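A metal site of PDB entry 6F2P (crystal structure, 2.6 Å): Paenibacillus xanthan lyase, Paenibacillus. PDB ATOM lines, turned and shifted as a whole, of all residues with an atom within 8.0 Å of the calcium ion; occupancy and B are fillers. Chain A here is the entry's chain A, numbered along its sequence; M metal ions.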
ATOM      1  N   VAL A 909       3.347  -6.552  14.173  1.00  0.00           N
ATOM      2  CA  VAL A 909       3.437  -5.555  13.107  1.00  0.00           C
ATOM      3  C   VAL A 909       4.853  -5.504  12.546  1.00  0.00           C
ATOM      4  O   VAL A 909       5.800  -5.229  13.282  1.00  0.00           O
ATOM      5  CB  VAL A 909       3.005  -4.171  13.582  1.00  0.00           C
ATOM      6  CG1 VAL A 909       2.868  -3.239  12.398  1.00  0.00           C
ATOM      7  CG2 VAL A 909       1.688  -4.256  14.332  1.00  0.00           C
ATOM      8  N   ASP A 910       4.994  -5.785  11.252  1.00  0.00           N
ATOM      9  CA  ASP A 910       6.295  -5.744  10.583  1.00  0.00           C
ATOM     10  C   ASP A 910       6.409  -4.403   9.859  1.00  0.00           C
ATOM     11  O   ASP A 910       5.412  -3.710   9.701  1.00  0.00           O
ATOM     12  CB  ASP A 910       6.410  -6.906   9.591  1.00  0.00           C
ATOM     13  CG  ASP A 910       7.850  -7.135   9.137  1.00  0.00           C
ATOM     14  OD1 ASP A 910       8.657  -7.609   9.966  1.00  0.00           O
ATOM     15  OD2 ASP A 910       8.158  -6.848   7.964  1.00  0.00           O
ATOM     16  N   ASN A 911       7.617  -4.041   9.445  1.00  0.00           N
ATOM     17  CA  ASN A 911       7.807  -2.755   8.761  1.00  0.00           C
ATOM     18  C   ASN A 911       7.132  -2.727   7.398  1.00  0.00           C
ATOM     19  O   ASN A 911       6.843  -1.659   6.848  1.00  0.00           O
ATOM     20  CB  ASN A 911       9.284  -2.440   8.617  1.00  0.00           C
ATOM     21  CG  ASN A 911      10.039  -3.570   7.980  1.00  0.00           C
ATOM     22  OD1 ASN A 911      10.270  -4.604   8.596  1.00  0.00           O
ATOM     23  ND2 ASN A 911      10.436  -3.385   6.721  1.00  0.00           N
ATOM     24  N   ALA A 912       6.880  -3.918   6.849  1.00  0.00           N
ATOM     25  CA  ALA A 912       6.123  -4.063   5.612  1.00  0.00           C
ATOM     26  C   ALA A 912       5.657  -5.506   5.475  1.00  0.00           C
ATOM     27  O   ALA A 912       6.476  -6.354   5.152  1.00  0.00           O
ATOM     28  CB  ALA A 912       6.978  -3.686   4.411  1.00  0.00           C
ATOM     29  N   ASP A 913       4.384  -5.824   5.738  1.00  0.00           N
ATOM     30  CA  ASP A 913       3.289  -4.973   6.256  1.00  0.00           C
ATOM     31  C   ASP A 913       2.751  -3.778   5.479  1.00  0.00           C
ATOM     32  O   ASP A 913       3.461  -2.807   5.200  1.00  0.00           O
ATOM     33  CB  ASP A 913       3.418  -4.675   7.753  1.00  0.00           C
ATOM     34  CG  ASP A 913       2.962  -5.843   8.616  1.00  0.00           C
ATOM     35  OD1 ASP A 913       3.207  -6.997   8.227  1.00  0.00           O
ATOM     36  OD2 ASP A 913       2.340  -5.590   9.671  1.00  0.00           O
ATOM     37  N   THR A 926      16.954  -3.559   3.728  1.00  0.00           N
ATOM     38  CA  THR A 926      17.969  -4.517   3.271  1.00  0.00           C
ATOM     39  C   THR A 926      17.795  -5.927   3.853  1.00  0.00           C
ATOM     40  O   THR A 926      16.980  -6.149   4.755  1.00  0.00           O
ATOM     41  CB  THR A 926      19.406  -3.991   3.544  1.00  0.00           C
ATOM     42  OG1 THR A 926      20.346  -4.685   2.713  1.00  0.00           O
ATOM     43  CG2 THR A 926      19.796  -4.159   4.998  1.00  0.00           C
ATOM     44  N   ASP A 931      18.856 -10.825  11.043  1.00  0.00           N
ATOM     45  CA  ASP A 931      18.499 -10.599  12.436  1.00  0.00           C
ATOM     46  C   ASP A 931      16.989 -10.485  12.523  1.00  0.00           C
ATOM     47  O   ASP A 931      16.440  -9.908  13.460  1.00  0.00           O
ATOM     48  CB  ASP A 931      19.181  -9.363  12.995  1.00  0.00           C
ATOM     49  CG  ASP A 931      20.352  -9.702  13.895  1.00  0.00           C
ATOM     50  OD1 ASP A 931      20.451 -10.863  14.347  1.00  0.00           O
ATOM     51  OD2 ASP A 931      21.183  -8.798  14.151  1.00  0.00           O
ATOM     52  N   ARG A 932      16.341 -11.002  11.491  1.00  0.00           N
ATOM     53  CA  ARG A 932      14.985 -11.550  11.556  1.00  0.00           C
ATOM     54  C   ARG A 932      13.808 -10.596  11.350  1.00  0.00           C
ATOM     55  O   ARG A 932      13.945  -9.482  10.831  1.00  0.00           O
ATOM     56  CB  ARG A 932      14.784 -12.392  12.832  1.00  0.00           C
ATOM     57  CG  ARG A 932      15.856 -13.459  13.083  1.00  0.00           C
ATOM     58  CD  ARG A 932      15.360 -14.857  12.803  1.00  0.00           C
ATOM     59  NE  ARG A 932      14.121 -15.150  13.513  1.00  0.00           N
ATOM     60  CZ  ARG A 932      12.979 -15.451  12.920  1.00  0.00           C
ATOM     61  NH1 ARG A 932      12.922 -15.496  11.586  1.00  0.00           N
ATOM     62  NH2 ARG A 932      11.894 -15.703  13.630  1.00  0.00           N
ATOM     63  N   TYR A 933      12.655 -11.083  11.795  1.00  0.00           N
ATOM     64  CA  TYR A 933      11.331 -10.654  11.368  1.00  0.00           C
ATOM     65  C   TYR A 933      11.065 -10.114   9.967  1.00  0.00           C
ATOM     66  O   TYR A 933      11.378  -8.965   9.628  1.00  0.00           O
ATOM     67  CB  TYR A 933      10.487  -9.974  12.457  1.00  0.00           C
ATOM     68  CG  TYR A 933       9.111 -10.599  12.441  1.00  0.00           C
ATOM     69  CD1 TYR A 933       8.842 -11.749  13.169  1.00  0.00           C
ATOM     70  CD2 TYR A 933       8.120 -10.084  11.609  1.00  0.00           C
ATOM     71  CE1 TYR A 933       7.583 -12.343  13.125  1.00  0.00           C
ATOM     72  CE2 TYR A 933       6.875 -10.662  11.557  1.00  0.00           C
ATOM     73  CZ  TYR A 933       6.604 -11.789  12.304  1.00  0.00           C
ATOM     74  OH  TYR A 933       5.353 -12.362  12.240  1.00  0.00           O
ATOM     75  N   GLY A 934      10.427 -10.985   9.177  1.00  0.00           N
ATOM     76  CA  GLY A 934      10.110 -10.726   7.784  1.00  0.00           C
ATOM     77  C   GLY A 934      11.302 -11.017   6.889  1.00  0.00           C
ATOM     78  O   GLY A 934      12.271 -11.652   7.303  1.00  0.00           O
ATOM     79  N   ALA A 935      11.238 -10.532   5.660  1.00  0.00           N
ATOM     80  CA  ALA A 935      12.383 -10.584   4.769  1.00  0.00           C
ATOM     81  C   ALA A 935      13.407  -9.561   5.223  1.00  0.00           C
ATOM     82  O   ALA A 935      14.557  -9.897   5.513  1.00  0.00           O
ATOM     83  CB  ALA A 935      11.940 -10.286   3.345  1.00  0.00           C
ATOM     84  N   ASP A 936      12.949  -8.323   5.323  1.00  0.00           N
ATOM     85  CA  ASP A 936      13.824  -7.172   5.459  1.00  0.00           C
ATOM     86  C   ASP A 936      13.639  -6.426   6.783  1.00  0.00           C
ATOM     87  O   ASP A 936      12.833  -6.832   7.637  1.00  0.00           O
ATOM     88  CB  ASP A 936      13.556  -6.201   4.305  1.00  0.00           C
ATOM     89  CG  ASP A 936      12.133  -5.633   4.328  1.00  0.00           C
ATOM     90  OD1 ASP A 936      11.285  -6.126   5.108  1.00  0.00           O
ATOM     91  OD2 ASP A 936      11.851  -4.696   3.553  1.00  0.00           O
ATOM     92  N   TYR A 937      14.414  -5.355   6.942  1.00  0.00           N
ATOM     93  CA  TYR A 937      14.203  -4.349   7.976  1.00  0.00           C
ATOM     94  C   TYR A 937      14.572  -2.997   7.358  1.00  0.00           C
ATOM     95  O   TYR A 937      15.065  -2.962   6.233  1.00  0.00           O
ATOM     96  CB  TYR A 937      15.073  -4.619   9.194  1.00  0.00           C
ATOM     97  CG  TYR A 937      16.518  -4.948   8.882  1.00  0.00           C
ATOM     98  CD1 TYR A 937      17.458  -3.949   8.703  1.00  0.00           C
ATOM     99  CD2 TYR A 937      16.935  -6.267   8.768  1.00  0.00           C
ATOM    100  CE1 TYR A 937      18.774  -4.254   8.422  1.00  0.00           C
ATOM    101  CE2 TYR A 937      18.245  -6.580   8.486  1.00  0.00           C
ATOM    102  CZ  TYR A 937      19.161  -5.577   8.313  1.00  0.00           C
ATOM    103  OH  TYR A 937      20.474  -5.890   8.021  1.00  0.00           O
ATOM    104  N   ILE A 938      14.326  -1.903   8.059  1.00  0.00           N
ATOM    105  CA  ILE A 938      14.677  -0.595   7.533  1.00  0.00           C
ATOM    106  C   ILE A 938      15.603   0.189   8.465  1.00  0.00           C
ATOM    107  O   ILE A 938      15.701  -0.122   9.648  1.00  0.00           O
ATOM    108  CB  ILE A 938      13.416   0.235   7.174  1.00  0.00           C
ATOM    109  CG1 ILE A 938      12.481   0.362   8.364  1.00  0.00           C
ATOM    110  CG2 ILE A 938      12.686  -0.397   6.008  1.00  0.00           C
ATOM    111  CD1 ILE A 938      11.280   1.240   8.097  1.00  0.00           C
ATOM    112  N   PHE A 952       4.533   1.960  14.595  1.00  0.00           N
ATOM    113  CA  PHE A 952       3.761   0.719  14.540  1.00  0.00           C
ATOM    114  C   PHE A 952       2.426   0.853  15.281  1.00  0.00           C
ATOM    115  O   PHE A 952       2.409   0.910  16.506  1.00  0.00           O
ATOM    116  CB  PHE A 952       4.542  -0.436  15.174  1.00  0.00           C
ATOM    117  CG  PHE A 952       5.883  -0.717  14.537  1.00  0.00           C
ATOM    118  CD1 PHE A 952       7.029  -0.065  14.963  1.00  0.00           C
ATOM    119  CD2 PHE A 952       5.997  -1.657  13.519  1.00  0.00           C
ATOM    120  CE1 PHE A 952       8.258  -0.336  14.393  1.00  0.00           C
ATOM    121  CE2 PHE A 952       7.229  -1.929  12.940  1.00  0.00           C
ATOM    122  CZ  PHE A 952       8.371  -1.263  13.373  1.00  0.00           C
ATOM    123  N   MET A 967      11.751  -6.476  17.989  1.00  0.00           N
ATOM    124  CA  MET A 967      12.897  -7.150  17.419  1.00  0.00           C
ATOM    125  C   MET A 967      13.595  -6.189  16.470  1.00  0.00           C
ATOM    126  O   MET A 967      12.950  -5.290  15.915  1.00  0.00           O
ATOM    127  CB  MET A 967      12.449  -8.396  16.666  1.00  0.00           C
ATOM    128  CG  MET A 967      13.570  -9.208  16.058  1.00  0.00           C
ATOM    129  SD  MET A 967      12.908 -10.724  15.348  1.00  0.00           S
ATOM    130  CE  MET A 967      12.244 -11.509  16.816  1.00  0.00           C
ATOM    131  N   ALA A1031      14.446  -0.161  12.278  1.00  0.00           N
ATOM    132  CA  ALA A1031      13.033  -0.435  12.567  1.00  0.00           C
ATOM    133  C   ALA A1031      12.642  -1.779  11.947  1.00  0.00           C
ATOM    134  O   ALA A1031      12.830  -1.978  10.740  1.00  0.00           O
ATOM    135  CB  ALA A1031      12.139   0.682  12.024  1.00  0.00           C
ATOM    136  N   ASP A1032      12.097  -2.687  12.752  1.00  0.00           N
ATOM    137  CA  ASP A1032      11.786  -4.038  12.283  1.00  0.00           C
ATOM    138  C   ASP A1032      10.361  -4.476  12.612  1.00  0.00           C
ATOM    139  O   ASP A1032       9.455  -4.359  11.776  1.00  0.00           O
ATOM    140  CB  ASP A1032      12.811  -5.038  12.837  1.00  0.00           C
ATOM    141  CG  ASP A1032      12.692  -6.423  12.219  1.00  0.00           C
ATOM    142  OD1 ASP A1032      12.169  -6.531  11.094  1.00  0.00           O
ATOM    143  OD2 ASP A1032      13.149  -7.394  12.860  1.00  0.00           O
ATOM    144  N   ALA A1033      10.142  -4.973  13.830  1.00  0.00           N
ATOM    145  CA  ALA A1033       8.831  -5.471  14.230  1.00  0.00           C
ATOM    146  C   ALA A1033       8.516  -5.356  15.733  1.00  0.00           C
ATOM    147  O   ALA A1033       9.411  -5.430  16.585  1.00  0.00           O
ATOM    148  CB  ALA A1033       8.635  -6.911  13.752  1.00  0.00           C
HETATM  149 CA    CA M   1      10.863  -6.787   8.962  1.00  0.00          CA
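N of Tyr 933 sits at hydrogen-bond distance from SD of Met 967. The side-chain carboxylate (OD2) of Asp 910 sits close to the backbone NH (N) of Ala 912, 3.4 Å away. The side-chain carboxylate (OD2) of Asp 913 is in hydrogen-bond range of the backbone NH (N) of Asp 910, 3.1 Å away.
Five residues have an atom within 4 Å of the calcium ion: Asp 910, Asn 911, Tyr 933, Asp 936 and Asp 1032. Along chain A the residues within 4 Å of the calcium ion span positions 910 to 1032. The nearest printed residue that does not touch the calcium ion is Gly 934 (4.2 Å).
The calcium ion is bound by OD1 of Asn 911 (2.3 Å), O of Tyr 933 (2.3 Å), O of Asp 936 (2.4 Å), OD1 of Asp 1032 (2.5 Å), OD1 of Asp 910 (2.6 Å) and OD2 of Asp 910 (2.9 Å). The calcium ion has six donor atoms within binding distance.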
